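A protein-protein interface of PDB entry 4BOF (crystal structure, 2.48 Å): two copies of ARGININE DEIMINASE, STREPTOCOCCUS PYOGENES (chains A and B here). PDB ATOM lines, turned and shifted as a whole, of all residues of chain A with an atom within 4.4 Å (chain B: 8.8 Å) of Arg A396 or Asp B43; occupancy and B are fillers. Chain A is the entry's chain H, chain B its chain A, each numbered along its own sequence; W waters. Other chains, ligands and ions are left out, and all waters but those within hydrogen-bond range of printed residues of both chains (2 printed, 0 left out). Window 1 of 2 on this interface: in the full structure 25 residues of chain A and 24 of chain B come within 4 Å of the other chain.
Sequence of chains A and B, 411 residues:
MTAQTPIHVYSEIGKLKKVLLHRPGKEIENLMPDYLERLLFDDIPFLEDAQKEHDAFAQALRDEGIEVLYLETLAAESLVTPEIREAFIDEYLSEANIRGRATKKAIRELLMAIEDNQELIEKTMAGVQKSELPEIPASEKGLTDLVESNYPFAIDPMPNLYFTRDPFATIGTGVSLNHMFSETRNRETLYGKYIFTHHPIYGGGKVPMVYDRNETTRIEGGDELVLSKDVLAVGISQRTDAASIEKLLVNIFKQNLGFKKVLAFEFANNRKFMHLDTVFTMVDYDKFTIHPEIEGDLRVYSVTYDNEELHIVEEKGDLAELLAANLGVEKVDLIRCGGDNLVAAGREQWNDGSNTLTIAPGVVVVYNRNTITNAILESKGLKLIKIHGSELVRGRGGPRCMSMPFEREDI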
ATOM      1  N   ASP A  42       1.060  -3.402 -12.750  1.00  0.00           N
ATOM      2  CA  ASP A  42       0.337  -2.220 -13.242  1.00  0.00           C
ATOM      3  C   ASP A  42       1.251  -1.022 -13.483  1.00  0.00           C
ATOM      4  O   ASP A  42       0.976  -0.195 -14.354  1.00  0.00           O
ATOM      5  CB  ASP A  42      -0.784  -1.824 -12.269  1.00  0.00           C
ATOM      6  CG  ASP A  42      -2.049  -2.617 -12.516  1.00  0.00           C
ATOM      7  OD1 ASP A  42      -2.098  -3.812 -12.110  1.00  0.00           O
ATOM      8  OD2 ASP A  42      -2.947  -2.088 -13.188  1.00  0.00           O
ATOM      9  N   ASP A  43       2.316  -0.923 -12.712  1.00  0.00           N
ATOM     10  CA  ASP A  43       3.265   0.168 -12.816  1.00  0.00           C
ATOM     11  C   ASP A  43       4.644  -0.321 -12.335  1.00  0.00           C
ATOM     12  O   ASP A  43       4.752  -1.421 -11.789  1.00  0.00           O
ATOM     13  CB  ASP A  43       2.759   1.369 -11.988  1.00  0.00           C
ATOM     14  CG  ASP A  43       3.248   2.744 -12.420  1.00  0.00           C
ATOM     15  OD1 ASP A  43       4.403   2.848 -12.903  1.00  0.00           O
ATOM     16  OD2 ASP A  43       2.499   3.725 -12.226  1.00  0.00           O
ATOM     17  N   PHE A 163       4.156 -11.009  -2.842  1.00  0.00           N
ATOM     18  CA  PHE A 163       2.769 -11.458  -2.631  1.00  0.00           C
ATOM     19  C   PHE A 163       2.801 -12.977  -2.353  1.00  0.00           C
ATOM     20  O   PHE A 163       2.565 -13.799  -3.264  1.00  0.00           O
ATOM     21  CB  PHE A 163       1.827 -11.118  -3.806  1.00  0.00           C
ATOM     22  CG  PHE A 163       1.725  -9.663  -4.142  1.00  0.00           C
ATOM     23  CD1 PHE A 163       1.218  -8.751  -3.216  1.00  0.00           C
ATOM     24  CD2 PHE A 163       2.065  -9.205  -5.410  1.00  0.00           C
ATOM     25  CE1 PHE A 163       1.098  -7.404  -3.540  1.00  0.00           C
ATOM     26  CE2 PHE A 163       1.959  -7.850  -5.730  1.00  0.00           C
ATOM     27  CZ  PHE A 163       1.457  -6.963  -4.801  1.00  0.00           C
ATOM     28  N   MET A 274     -10.040 -11.526  -9.671  1.00  0.00           N
ATOM     29  CA  MET A 274      -9.098 -12.635  -9.745  1.00  0.00           C
ATOM     30  C   MET A 274      -9.300 -13.681  -8.639  1.00  0.00           C
ATOM     31  O   MET A 274      -9.417 -14.870  -8.956  1.00  0.00           O
ATOM     32  CB  MET A 274      -7.637 -12.124  -9.754  1.00  0.00           C
ATOM     33  CG  MET A 274      -7.344 -11.015  -8.738  1.00  0.00           C
ATOM     34  SD  MET A 274      -5.624 -10.430  -8.728  1.00  0.00           S
ATOM     35  CE  MET A 274      -5.731  -9.106  -7.537  1.00  0.00           C
ATOM     36  N   TRP A 350     -10.039  -1.696  -6.214  1.00  0.00           N
ATOM     37  CA  TRP A 350      -8.842  -1.719  -7.041  1.00  0.00           C
ATOM     38  C   TRP A 350      -7.555  -1.622  -6.195  1.00  0.00           C
ATOM     39  O   TRP A 350      -6.531  -2.225  -6.560  1.00  0.00           O
ATOM     40  CB  TRP A 350      -8.938  -0.553  -8.014  1.00  0.00           C
ATOM     41  CG  TRP A 350      -7.724  -0.301  -8.850  1.00  0.00           C
ATOM     42  CD1 TRP A 350      -6.807   0.689  -8.676  1.00  0.00           C
ATOM     43  CD2 TRP A 350      -7.361  -0.980 -10.058  1.00  0.00           C
ATOM     44  NE1 TRP A 350      -5.879   0.660  -9.692  1.00  0.00           N
ATOM     45  CE2 TRP A 350      -6.193  -0.356 -10.553  1.00  0.00           C
ATOM     46  CE3 TRP A 350      -7.890  -2.076 -10.756  1.00  0.00           C
ATOM     47  CZ2 TRP A 350      -5.570  -0.764 -11.736  1.00  0.00           C
ATOM     48  CZ3 TRP A 350      -7.268  -2.486 -11.931  1.00  0.00           C
ATOM     49  CH2 TRP A 350      -6.108  -1.851 -12.394  1.00  0.00           C
ATOM     50  N   ASN A 351      -7.617  -0.875  -5.069  1.00  0.00           N
ATOM     51  CA  ASN A 351      -6.502  -0.695  -4.140  1.00  0.00           C
ATOM     52  C   ASN A 351      -6.517  -1.720  -2.994  1.00  0.00           C
ATOM     53  O   ASN A 351      -5.878  -1.497  -1.971  1.00  0.00           O
ATOM     54  CB  ASN A 351      -6.486   0.729  -3.588  1.00  0.00           C
ATOM     55  CG  ASN A 351      -6.079   1.765  -4.597  1.00  0.00           C
ATOM     56  OD1 ASN A 351      -6.642   2.845  -4.663  1.00  0.00           O
ATOM     57  ND2 ASN A 351      -5.088   1.473  -5.404  1.00  0.00           N
ATOM     58  N   ASP A 352      -7.197  -2.873  -3.207  1.00  0.00           N
ATOM     59  CA  ASP A 352      -7.359  -4.043  -2.316  1.00  0.00           C
ATOM     60  C   ASP A 352      -8.053  -3.718  -0.972  1.00  0.00           C
ATOM     61  O   ASP A 352      -7.815  -4.399   0.030  1.00  0.00           O
ATOM     62  CB  ASP A 352      -6.017  -4.759  -2.083  1.00  0.00           C
ATOM     63  CG  ASP A 352      -5.665  -5.661  -3.238  1.00  0.00           C
ATOM     64  OD1 ASP A 352      -5.088  -5.150  -4.223  1.00  0.00           O
ATOM     65  OD2 ASP A 352      -6.076  -6.848  -3.212  1.00  0.00           O
ATOM     66  N   VAL A 393       1.382  -1.146  -3.654  1.00  0.00           N
ATOM     67  CA  VAL A 393       0.076  -1.319  -4.296  1.00  0.00           C
ATOM     68  C   VAL A 393       0.188  -1.360  -5.823  1.00  0.00           C
ATOM     69  O   VAL A 393      -0.782  -1.719  -6.449  1.00  0.00           O
ATOM     70  CB  VAL A 393      -0.971  -0.278  -3.847  1.00  0.00           C
ATOM     71  CG1 VAL A 393      -0.723   1.093  -4.508  1.00  0.00           C
ATOM     72  CG2 VAL A 393      -2.386  -0.792  -4.132  1.00  0.00           C
ATOM     73  N   ARG A 394       1.330  -1.000  -6.408  1.00  0.00           N
ATOM     74  CA  ARG A 394       1.576  -1.033  -7.855  1.00  0.00           C
ATOM     75  C   ARG A 394       1.507  -2.478  -8.411  1.00  0.00           C
ATOM     76  O   ARG A 394       1.129  -2.673  -9.564  1.00  0.00           O
ATOM     77  CB  ARG A 394       2.908  -0.377  -8.214  1.00  0.00           C
ATOM     78  CG  ARG A 394       2.815   1.146  -8.220  1.00  0.00           C
ATOM     79  CD  ARG A 394       4.113   1.818  -8.600  1.00  0.00           C
ATOM     80  NE  ARG A 394       4.389   2.896  -7.659  1.00  0.00           N
ATOM     81  CZ  ARG A 394       4.267   4.190  -7.915  1.00  0.00           C
ATOM     82  NH1 ARG A 394       3.960   4.607  -9.123  1.00  0.00           N
ATOM     83  NH2 ARG A 394       4.506   5.075  -6.972  1.00  0.00           N
ATOM     84  N   GLY A 395       1.786  -3.456  -7.556  1.00  0.00           N
ATOM     85  CA  GLY A 395       1.701  -4.868  -7.870  1.00  0.00           C
ATOM     86  C   GLY A 395       0.286  -5.408  -7.767  1.00  0.00           C
ATOM     87  O   GLY A 395       0.079  -6.602  -7.965  1.00  0.00           O
ATOM     88  N   ARG A 396      -0.703  -4.527  -7.475  1.00  0.00           N
ATOM     89  CA  ARG A 396      -2.145  -4.817  -7.395  1.00  0.00           C
ATOM     90  C   ARG A 396      -2.459  -5.871  -6.305  1.00  0.00           C
ATOM     91  O   ARG A 396      -3.114  -6.893  -6.580  1.00  0.00           O
ATOM     92  CB  ARG A 396      -2.708  -5.245  -8.795  1.00  0.00           C
ATOM     93  CG  ARG A 396      -4.183  -4.855  -9.035  1.00  0.00           C
ATOM     94  CD  ARG A 396      -4.482  -3.409  -9.438  1.00  0.00           C
ATOM     95  NE  ARG A 396      -4.184  -2.382  -8.425  1.00  0.00           N
ATOM     96  CZ  ARG A 396      -3.387  -1.330  -8.622  1.00  0.00           C
ATOM     97  NH1 ARG A 396      -2.779  -1.155  -9.786  1.00  0.00           N
ATOM     98  NH2 ARG A 396      -3.195  -0.447  -7.656  1.00  0.00           N
ATOM     99  N   GLY A 397      -2.000  -5.596  -5.081  1.00  0.00           N
ATOM    100  CA  GLY A 397      -2.218  -6.447  -3.917  1.00  0.00           C
ATOM    101  C   GLY A 397      -1.984  -5.665  -2.639  1.00  0.00           C
ATOM    102  O   GLY A 397      -1.139  -4.766  -2.587  1.00  0.00           O
ATOM    103  N   ILE B  28      -9.167  13.457  -9.746  1.00  0.00           N
ATOM    104  CA  ILE B  28      -8.317  12.302  -9.472  1.00  0.00           C
ATOM    105  C   ILE B  28      -9.112  11.272  -8.662  1.00  0.00           C
ATOM    106  O   ILE B  28      -8.858  10.070  -8.779  1.00  0.00           O
ATOM    107  CB  ILE B  28      -7.036  12.815  -8.735  1.00  0.00           C
ATOM    108  CG1 ILE B  28      -6.125  13.679  -9.656  1.00  0.00           C
ATOM    109  CG2 ILE B  28      -6.244  11.721  -8.017  1.00  0.00           C
ATOM    110  CD1 ILE B  28      -5.797  13.093 -10.987  1.00  0.00           C
ATOM    111  N   LEU B  31     -11.741   8.790 -10.642  1.00  0.00           N
ATOM    112  CA  LEU B  31     -11.141   7.804 -11.533  1.00  0.00           C
ATOM    113  C   LEU B  31     -11.630   6.431 -11.097  1.00  0.00           C
ATOM    114  O   LEU B  31     -11.776   6.169  -9.907  1.00  0.00           O
ATOM    115  CB  LEU B  31      -9.607   7.889 -11.539  1.00  0.00           C
ATOM    116  CG  LEU B  31      -8.994   9.017 -12.357  1.00  0.00           C
ATOM    117  CD1 LEU B  31      -7.503   9.193 -12.067  1.00  0.00           C
ATOM    118  CD2 LEU B  31      -9.162   8.755 -13.827  1.00  0.00           C
ATOM    119  N   MET B  32     -11.950   5.581 -12.059  1.00  0.00           N
ATOM    120  CA  MET B  32     -12.434   4.236 -11.824  1.00  0.00           C
ATOM    121  C   MET B  32     -11.655   3.269 -12.694  1.00  0.00           C
ATOM    122  O   MET B  32     -11.270   3.654 -13.804  1.00  0.00           O
ATOM    123  CB  MET B  32     -13.928   4.149 -12.108  1.00  0.00           C
ATOM    124  CG  MET B  32     -14.768   4.654 -10.978  1.00  0.00           C
ATOM    125  SD  MET B  32     -16.456   4.086 -11.198  1.00  0.00           S
ATOM    126  CE  MET B  32     -16.348   2.410 -10.554  1.00  0.00           C
ATOM    127  N   PRO B  33     -11.367   2.029 -12.200  1.00  0.00           N
ATOM    128  CA  PRO B  33     -10.539   1.082 -12.985  1.00  0.00           C
ATOM    129  C   PRO B  33     -11.013   0.807 -14.427  1.00  0.00           C
ATOM    130  O   PRO B  33     -10.206   0.893 -15.343  1.00  0.00           O
ATOM    131  CB  PRO B  33     -10.559  -0.203 -12.149  1.00  0.00           C
ATOM    132  CG  PRO B  33     -11.595  -0.001 -11.102  1.00  0.00           C
ATOM    133  CD  PRO B  33     -11.700   1.466 -10.876  1.00  0.00           C
ATOM    134  N   LEU B  36     -10.066   3.777 -17.048  1.00  0.00           N
ATOM    135  CA  LEU B  36      -8.712   4.334 -17.086  1.00  0.00           C
ATOM    136  C   LEU B  36      -8.289   4.445 -18.553  1.00  0.00           C
ATOM    137  O   LEU B  36      -7.261   5.062 -18.882  1.00  0.00           O
ATOM    138  CB  LEU B  36      -7.757   3.446 -16.268  1.00  0.00           C
ATOM    139  CG  LEU B  36      -7.336   3.899 -14.853  1.00  0.00           C
ATOM    140  CD1 LEU B  36      -8.385   4.767 -14.152  1.00  0.00           C
ATOM    141  CD2 LEU B  36      -7.027   2.704 -13.990  1.00  0.00           C
ATOM    142  N   LEU B  40      -7.070   9.131 -19.193  1.00  0.00           N
ATOM    143  CA  LEU B  40      -5.674   8.979 -19.655  1.00  0.00           C
ATOM    144  C   LEU B  40      -4.738   8.704 -18.495  1.00  0.00           C
ATOM    145  O   LEU B  40      -3.759   9.437 -18.291  1.00  0.00           O
ATOM    146  CB  LEU B  40      -5.187  10.219 -20.449  1.00  0.00           C
ATOM    147  CG  LEU B  40      -4.385   9.974 -21.759  1.00  0.00           C
ATOM    148  CD1 LEU B  40      -4.105  11.277 -22.491  1.00  0.00           C
ATOM    149  CD2 LEU B  40      -3.033   9.268 -21.503  1.00  0.00           C
ATOM    150  N   PHE B  41      -4.972   7.612 -17.761  1.00  0.00           N
ATOM    151  CA  PHE B  41      -4.152   7.364 -16.584  1.00  0.00           C
ATOM    152  C   PHE B  41      -3.621   5.941 -16.505  1.00  0.00           C
ATOM    153  O   PHE B  41      -4.296   5.022 -16.951  1.00  0.00           O
ATOM    154  CB  PHE B  41      -5.030   7.696 -15.388  1.00  0.00           C
ATOM    155  CG  PHE B  41      -4.631   8.987 -14.737  1.00  0.00           C
ATOM    156  CD1 PHE B  41      -4.815  10.198 -15.388  1.00  0.00           C
ATOM    157  CD2 PHE B  41      -4.027   8.990 -13.492  1.00  0.00           C
ATOM    158  CE1 PHE B  41      -4.373  11.382 -14.815  1.00  0.00           C
ATOM    159  CE2 PHE B  41      -3.619  10.178 -12.901  1.00  0.00           C
ATOM    160  CZ  PHE B  41      -3.796  11.367 -13.564  1.00  0.00           C
ATOM    161  N   ASP B  42      -2.408   5.762 -15.937  1.00  0.00           N
ATOM    162  CA  ASP B  42      -1.777   4.440 -15.790  1.00  0.00           C
ATOM    163  C   ASP B  42      -2.202   3.712 -14.507  1.00  0.00           C
ATOM    164  O   ASP B  42      -2.154   2.476 -14.459  1.00  0.00           O
ATOM    165  CB  ASP B  42      -0.244   4.552 -15.832  1.00  0.00           C
ATOM    166  CG  ASP B  42       0.291   4.561 -17.259  1.00  0.00           C
ATOM    167  OD1 ASP B  42       0.208   5.627 -17.921  1.00  0.00           O
ATOM    168  OD2 ASP B  42       0.712   3.489 -17.742  1.00  0.00           O
ATOM    169  N   ASP B  43      -2.561   4.478 -13.463  1.00  0.00           N
ATOM    170  CA  ASP B  43      -2.989   3.952 -12.174  1.00  0.00           C
ATOM    171  C   ASP B  43      -3.898   4.972 -11.503  1.00  0.00           C
ATOM    172  O   ASP B  43      -4.000   6.099 -11.974  1.00  0.00           O
ATOM    173  CB  ASP B  43      -1.762   3.610 -11.307  1.00  0.00           C
ATOM    174  CG  ASP B  43      -1.964   2.525 -10.258  1.00  0.00           C
ATOM    175  OD1 ASP B  43      -3.081   2.435  -9.698  1.00  0.00           O
ATOM    176  OD2 ASP B  43      -0.980   1.799  -9.952  1.00  0.00           O
ATOM    177  N   ILE B  44      -4.601   4.565 -10.451  1.00  0.00           N
ATOM    178  CA  ILE B  44      -5.493   5.434  -9.687  1.00  0.00           C
ATOM    179  C   ILE B  44      -4.685   6.004  -8.471  1.00  0.00           C
ATOM    180  O   ILE B  44      -4.282   5.246  -7.593  1.00  0.00           O
ATOM    181  CB  ILE B  44      -6.802   4.684  -9.282  1.00  0.00           C
ATOM    182  CG1 ILE B  44      -7.699   4.480 -10.502  1.00  0.00           C
ATOM    183  CG2 ILE B  44      -7.555   5.437  -8.184  1.00  0.00           C
ATOM    184  CD1 ILE B  44      -8.489   3.269 -10.524  1.00  0.00           C
ATOM    185  N   PRO B  45      -4.422   7.319  -8.425  1.00  0.00           N
ATOM    186  CA  PRO B  45      -3.630   7.872  -7.310  1.00  0.00           C
ATOM    187  C   PRO B  45      -4.436   8.067  -6.046  1.00  0.00           C
ATOM    188  O   PRO B  45      -5.652   8.124  -6.101  1.00  0.00           O
ATOM    189  CB  PRO B  45      -3.194   9.247  -7.836  1.00  0.00           C
ATOM    190  CG  PRO B  45      -3.614   9.286  -9.315  1.00  0.00           C
ATOM    191  CD  PRO B  45      -4.771   8.362  -9.406  1.00  0.00           C
ATOM    192  N   PHE B  46      -3.742   8.190  -4.900  1.00  0.00           N
ATOM    193  CA  PHE B  46      -4.337   8.556  -3.620  1.00  0.00           C
ATOM    194  C   PHE B  46      -4.281  10.100  -3.555  1.00  0.00           C
ATOM    195  O   PHE B  46      -3.217  10.682  -3.409  1.00  0.00           O
ATOM    196  CB  PHE B  46      -3.613   7.871  -2.457  1.00  0.00           C
ATOM    197  CG  PHE B  46      -4.043   8.245  -1.055  1.00  0.00           C
ATOM    198  CD1 PHE B  46      -5.365   8.554  -0.772  1.00  0.00           C
ATOM    199  CD2 PHE B  46      -3.140   8.204   0.006  1.00  0.00           C
ATOM    200  CE1 PHE B  46      -5.762   8.873   0.540  1.00  0.00           C
ATOM    201  CE2 PHE B  46      -3.545   8.508   1.309  1.00  0.00           C
ATOM    202  CZ  PHE B  46      -4.845   8.855   1.565  1.00  0.00           C
ATOM    203  N   PRO B 159      -8.717  14.306 -15.371  1.00  0.00           N
ATOM    204  CA  PRO B 159      -7.621  13.992 -14.411  1.00  0.00           C
ATOM    205  C   PRO B 159      -6.195  14.451 -14.804  1.00  0.00           C
ATOM    206  O   PRO B 159      -5.332  14.593 -13.918  1.00  0.00           O
ATOM    207  CB  PRO B 159      -7.699  12.474 -14.265  1.00  0.00           C
ATOM    208  CG  PRO B 159      -8.309  12.001 -15.517  1.00  0.00           C
ATOM    209  CD  PRO B 159      -9.274  13.077 -15.973  1.00  0.00           C
ATOM    210  N   TYR B 162      -3.373  18.378 -13.895  1.00  0.00           N
ATOM    211  CA  TYR B 162      -2.197  18.838 -13.134  1.00  0.00           C
ATOM    212  C   TYR B 162      -0.936  18.878 -13.996  1.00  0.00           C
ATOM    213  O   TYR B 162       0.110  19.341 -13.550  1.00  0.00           O
ATOM    214  CB  TYR B 162      -1.981  18.078 -11.803  1.00  0.00           C
ATOM    215  CG  TYR B 162      -1.637  16.612 -11.889  1.00  0.00           C
ATOM    216  CD1 TYR B 162      -2.632  15.653 -12.033  1.00  0.00           C
ATOM    217  CD2 TYR B 162      -0.323  16.172 -11.740  1.00  0.00           C
ATOM    218  CE1 TYR B 162      -2.324  14.300 -12.125  1.00  0.00           C
ATOM    219  CE2 TYR B 162      -0.009  14.813 -11.779  1.00  0.00           C
ATOM    220  CZ  TYR B 162      -1.018  13.880 -11.961  1.00  0.00           C
ATOM    221  OH  TYR B 162      -0.748  12.534 -11.980  1.00  0.00           O
ATOM    222  N   TRP B 350      10.262   5.960 -18.885  1.00  0.00           N
ATOM    223  CA  TRP B 350       8.891   5.746 -18.442  1.00  0.00           C
ATOM    224  C   TRP B 350       8.494   6.678 -17.291  1.00  0.00           C
ATOM    225  O   TRP B 350       7.335   7.092 -17.226  1.00  0.00           O
ATOM    226  CB  TRP B 350       8.764   4.290 -17.982  1.00  0.00           C
ATOM    227  CG  TRP B 350       7.438   3.894 -17.384  1.00  0.00           C
ATOM    228  CD1 TRP B 350       7.162   3.688 -16.063  1.00  0.00           C
ATOM    229  CD2 TRP B 350       6.256   3.536 -18.101  1.00  0.00           C
ATOM    230  NE1 TRP B 350       5.878   3.223 -15.915  1.00  0.00           N
ATOM    231  CE2 TRP B 350       5.286   3.150 -17.149  1.00  0.00           C
ATOM    232  CE3 TRP B 350       5.913   3.521 -19.461  1.00  0.00           C
ATOM    233  CZ2 TRP B 350       3.991   2.729 -17.518  1.00  0.00           C
ATOM    234  CZ3 TRP B 350       4.639   3.105 -19.828  1.00  0.00           C
ATOM    235  CH2 TRP B 350       3.697   2.708 -18.864  1.00  0.00           C
ATOM    236  N   SER B 390       5.652   9.697  -6.178  1.00  0.00           N
ATOM    237  CA  SER B 390       5.080   8.355  -6.190  1.00  0.00           C
ATOM    238  C   SER B 390       3.626   8.348  -6.666  1.00  0.00           C
ATOM    239  O   SER B 390       3.255   7.475  -7.453  1.00  0.00           O
ATOM    240  CB  SER B 390       5.151   7.761  -4.795  1.00  0.00           C
ATOM    241  OG  SER B 390       4.724   6.412  -4.809  1.00  0.00           O
ATOM    242  N   GLU B 391       2.806   9.320  -6.197  1.00  0.00           N
ATOM    243  CA  GLU B 391       1.397   9.452  -6.633  1.00  0.00           C
ATOM    244  C   GLU B 391       1.260  10.228  -7.942  1.00  0.00           C
ATOM    245  O   GLU B 391       0.528   9.779  -8.808  1.00  0.00           O
ATOM    246  CB  GLU B 391       0.528  10.107  -5.564  1.00  0.00           C
ATOM    247  CG  GLU B 391       0.510   9.372  -4.234  1.00  0.00           C
ATOM    248  CD  GLU B 391      -0.109   7.987  -4.187  1.00  0.00           C
ATOM    249  OE1 GLU B 391      -0.984   7.677  -5.023  1.00  0.00           O
ATOM    250  OE2 GLU B 391       0.229   7.234  -3.251  1.00  0.00           O
ATOM    251  N   LEU B 392       1.912  11.393  -8.077  1.00  0.00           N
ATOM    252  CA  LEU B 392       1.877  12.216  -9.299  1.00  0.00           C
ATOM    253  C   LEU B 392       2.411  11.500 -10.604  1.00  0.00           C
ATOM    254  O   LEU B 392       1.826  11.699 -11.672  1.00  0.00           O
ATOM    255  CB  LEU B 392       2.670  13.493  -9.077  1.00  0.00           C
ATOM    256  CG  LEU B 392       2.342  14.293  -7.819  1.00  0.00           C
ATOM    257  CD1 LEU B 392       3.381  15.409  -7.627  1.00  0.00           C
ATOM    258  CD2 LEU B 392       0.895  14.841  -7.880  1.00  0.00           C
ATOM    259  N   VAL B 393       3.470  10.664 -10.521  1.00  0.00           N
ATOM    260  CA  VAL B 393       4.021   9.951 -11.689  1.00  0.00           C
ATOM    261  C   VAL B 393       2.994   8.877 -12.220  1.00  0.00           C
ATOM    262  O   VAL B 393       3.164   8.379 -13.330  1.00  0.00           O
ATOM    263  CB  VAL B 393       5.445   9.357 -11.424  1.00  0.00           C
ATOM    264  CG1 VAL B 393       5.391   8.089 -10.586  1.00  0.00           C
ATOM    265  CG2 VAL B 393       6.193   9.104 -12.724  1.00  0.00           C
ATOM    266  N   ARG B 394       1.911   8.592 -11.478  1.00  0.00           N
ATOM    267  CA  ARG B 394       0.889   7.656 -11.959  1.00  0.00           C
ATOM    268  C   ARG B 394       0.202   8.219 -13.210  1.00  0.00           C
ATOM    269  O   ARG B 394      -0.326   7.473 -14.042  1.00  0.00           O
ATOM    270  CB  ARG B 394      -0.145   7.341 -10.847  1.00  0.00           C
ATOM    271  CG  ARG B 394       0.371   6.337  -9.849  1.00  0.00           C
ATOM    272  CD  ARG B 394      -0.620   5.987  -8.768  1.00  0.00           C
ATOM    273  NE  ARG B 394       0.066   5.992  -7.488  1.00  0.00           N
ATOM    274  CZ  ARG B 394       0.393   4.917  -6.788  1.00  0.00           C
ATOM    275  NH1 ARG B 394       0.019   3.710  -7.194  1.00  0.00           N
ATOM    276  NH2 ARG B 394       1.068   5.041  -5.656  1.00  0.00           N
ATOM    277  N   GLY B 395       0.308   9.527 -13.372  1.00  0.00           N
ATOM    278  CA  GLY B 395      -0.246  10.221 -14.520  1.00  0.00           C
ATOM    279  C   GLY B 395       0.700  10.176 -15.689  1.00  0.00           C
ATOM    280  O   GLY B 395       0.373  10.694 -16.743  1.00  0.00           O
ATOM    281  N   ARG B 396       1.893   9.609 -15.509  1.00  0.00           N
ATOM    282  CA  ARG B 396       2.899   9.419 -16.562  1.00  0.00           C
ATOM    283  C   ARG B 396       3.485  10.771 -17.032  1.00  0.00           C
ATOM    284  O   ARG B 396       3.601  11.029 -18.233  1.00  0.00           O
ATOM    285  CB  ARG B 396       2.304   8.628 -17.755  1.00  0.00           C
ATOM    286  CG  ARG B 396       3.269   7.703 -18.528  1.00  0.00           C
ATOM    287  CD  ARG B 396       3.825   6.408 -17.922  1.00  0.00           C
ATOM    288  NE  ARG B 396       3.270   5.935 -16.653  1.00  0.00           N
ATOM    289  CZ  ARG B 396       3.932   5.874 -15.497  1.00  0.00           C
ATOM    290  NH1 ARG B 396       5.174   6.333 -15.407  1.00  0.00           N
ATOM    291  NH2 ARG B 396       3.350   5.360 -14.423  1.00  0.00           N
HETATM  292  O   HOH W   1      -3.236   3.010  -6.757  1.00  0.00           O
HETATM  293  O   HOH W   2      -6.184   5.586  -4.583  1.00  0.00           O
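The indole nitrogen (NE1) of Trp B350 lies within hydrogen-bond range of the side-chain carboxylate (OD1) of Asp A43 (3.4 Å).
NH2 of Arg A394 lies within hydrogen-bond range of OG of Ser B390, at 2.6 Å.
NH1 of Arg A396 is in salt-bridge range of OD2 of Asp B43.
The side-chain carboxylate (OD1) of Asp B43 lies within hydrogen-bond range of the indole nitrogen (NE1) of Trp A350, at 3.3 Å.
The side-chain carboxylate (OD2) of Asp A43 lies within salt-bridge range of the guanidinium group (NH2) of Arg B396, at 2.9 Å.
O of Val B393 is in hydrogen-bond range of NH2 of Arg B396 (3.2 Å).
The backbone carbonyl oxygen (O) of Trp B350 sits at hydrogen-bond distance from the guanidinium group (NH1) of Arg B396.
The guanidinium group of Arg A396 is in salt-bridge range of the side-chain carboxylate of Asp A42 (3.5 Å).
N of Asp B42 is in hydrogen-bond range of O of Arg B394, 3.3 Å away.
The backbone carbonyl oxygen of Trp A350 lies within hydrogen-bond range of the guanidinium group of Arg A396.
The side-chain carboxylate (OD2) of Asp B43 is in salt-bridge range of the guanidinium group (NH1) of Arg B394 (3.5 Å).
Among the printed residues, pairs that only touch across the chains: Trp A350 with Pro B33 (3.5 Å), Trp A350 with Ile B44 (3.6 Å), Arg A394 with Arg B394 (3.7 Å) and Val A393 with Arg B394 (3.8 Å).
Of chain B, only Asp B43 (3.5 Å) comes within 4 Å of Arg A396.
Of chain A, only Trp A350 (3.3 Å) and Arg A396 (3.5 Å) come within 4 Å of Asp B43.
No residue of chain B comes within 4 Å of Gly A397.
Printed residues of chain B within 4 Å of Asp A43: Trp B350 (3.4 Å) and Arg B396 (2.9 Å).
Printed residues of chain B within 4 Å of Arg A394: Ser B390 (2.6 Å) and Arg B394 (3.7 Å).
Of the 12 printed residues of chain A, 5 touch a printed residue of chain B.
Hydrophobic or aromatic side chains of chain A that line the printed part of chain B: Trp A350 and Val A393.
Along chain A the printed residues that touch a printed residue of chain B span positions 43 to 396.
Hydrophobic or aromatic side chains of chain B within 4 Å of the printed part of chain A: Pro B33, Ile B44 and Trp B350.
Among the printed residues, Asp or Glu carboxylates within 4 Å of a Lys or Arg side-chain nitrogen of the other chain: Asp A43 with Arg B396 and Arg A396 with Asp B43.
Asp A43 touches Trp B350, and with the chains exchanged Trp A350 touches Asp B43.
Asp A43 touches Arg B396, and with the chains exchanged Arg A396 touches Asp B43.
Val A393 touches Arg B394, but with the chains exchanged Arg A394 does not touch Val B393 (4.04 Å).
Arg A394 touches its own counterpart, Arg B394.
7 positions are printed for both chains.
Water W1 lies within hydrogen-bond range of O of Ile B44 (2.6 Å), ND2 of Asn A351 (2.8 Å), OD1 of Asp B43 (3.0 Å) and NH1 of Arg B394 (3.4 Å).
Water W2 lies within hydrogen-bond range of the side-chain amide oxygen of Asn A351 (2.8 Å) and the backbone carbonyl oxygen of Pro B45 (3.0 Å).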
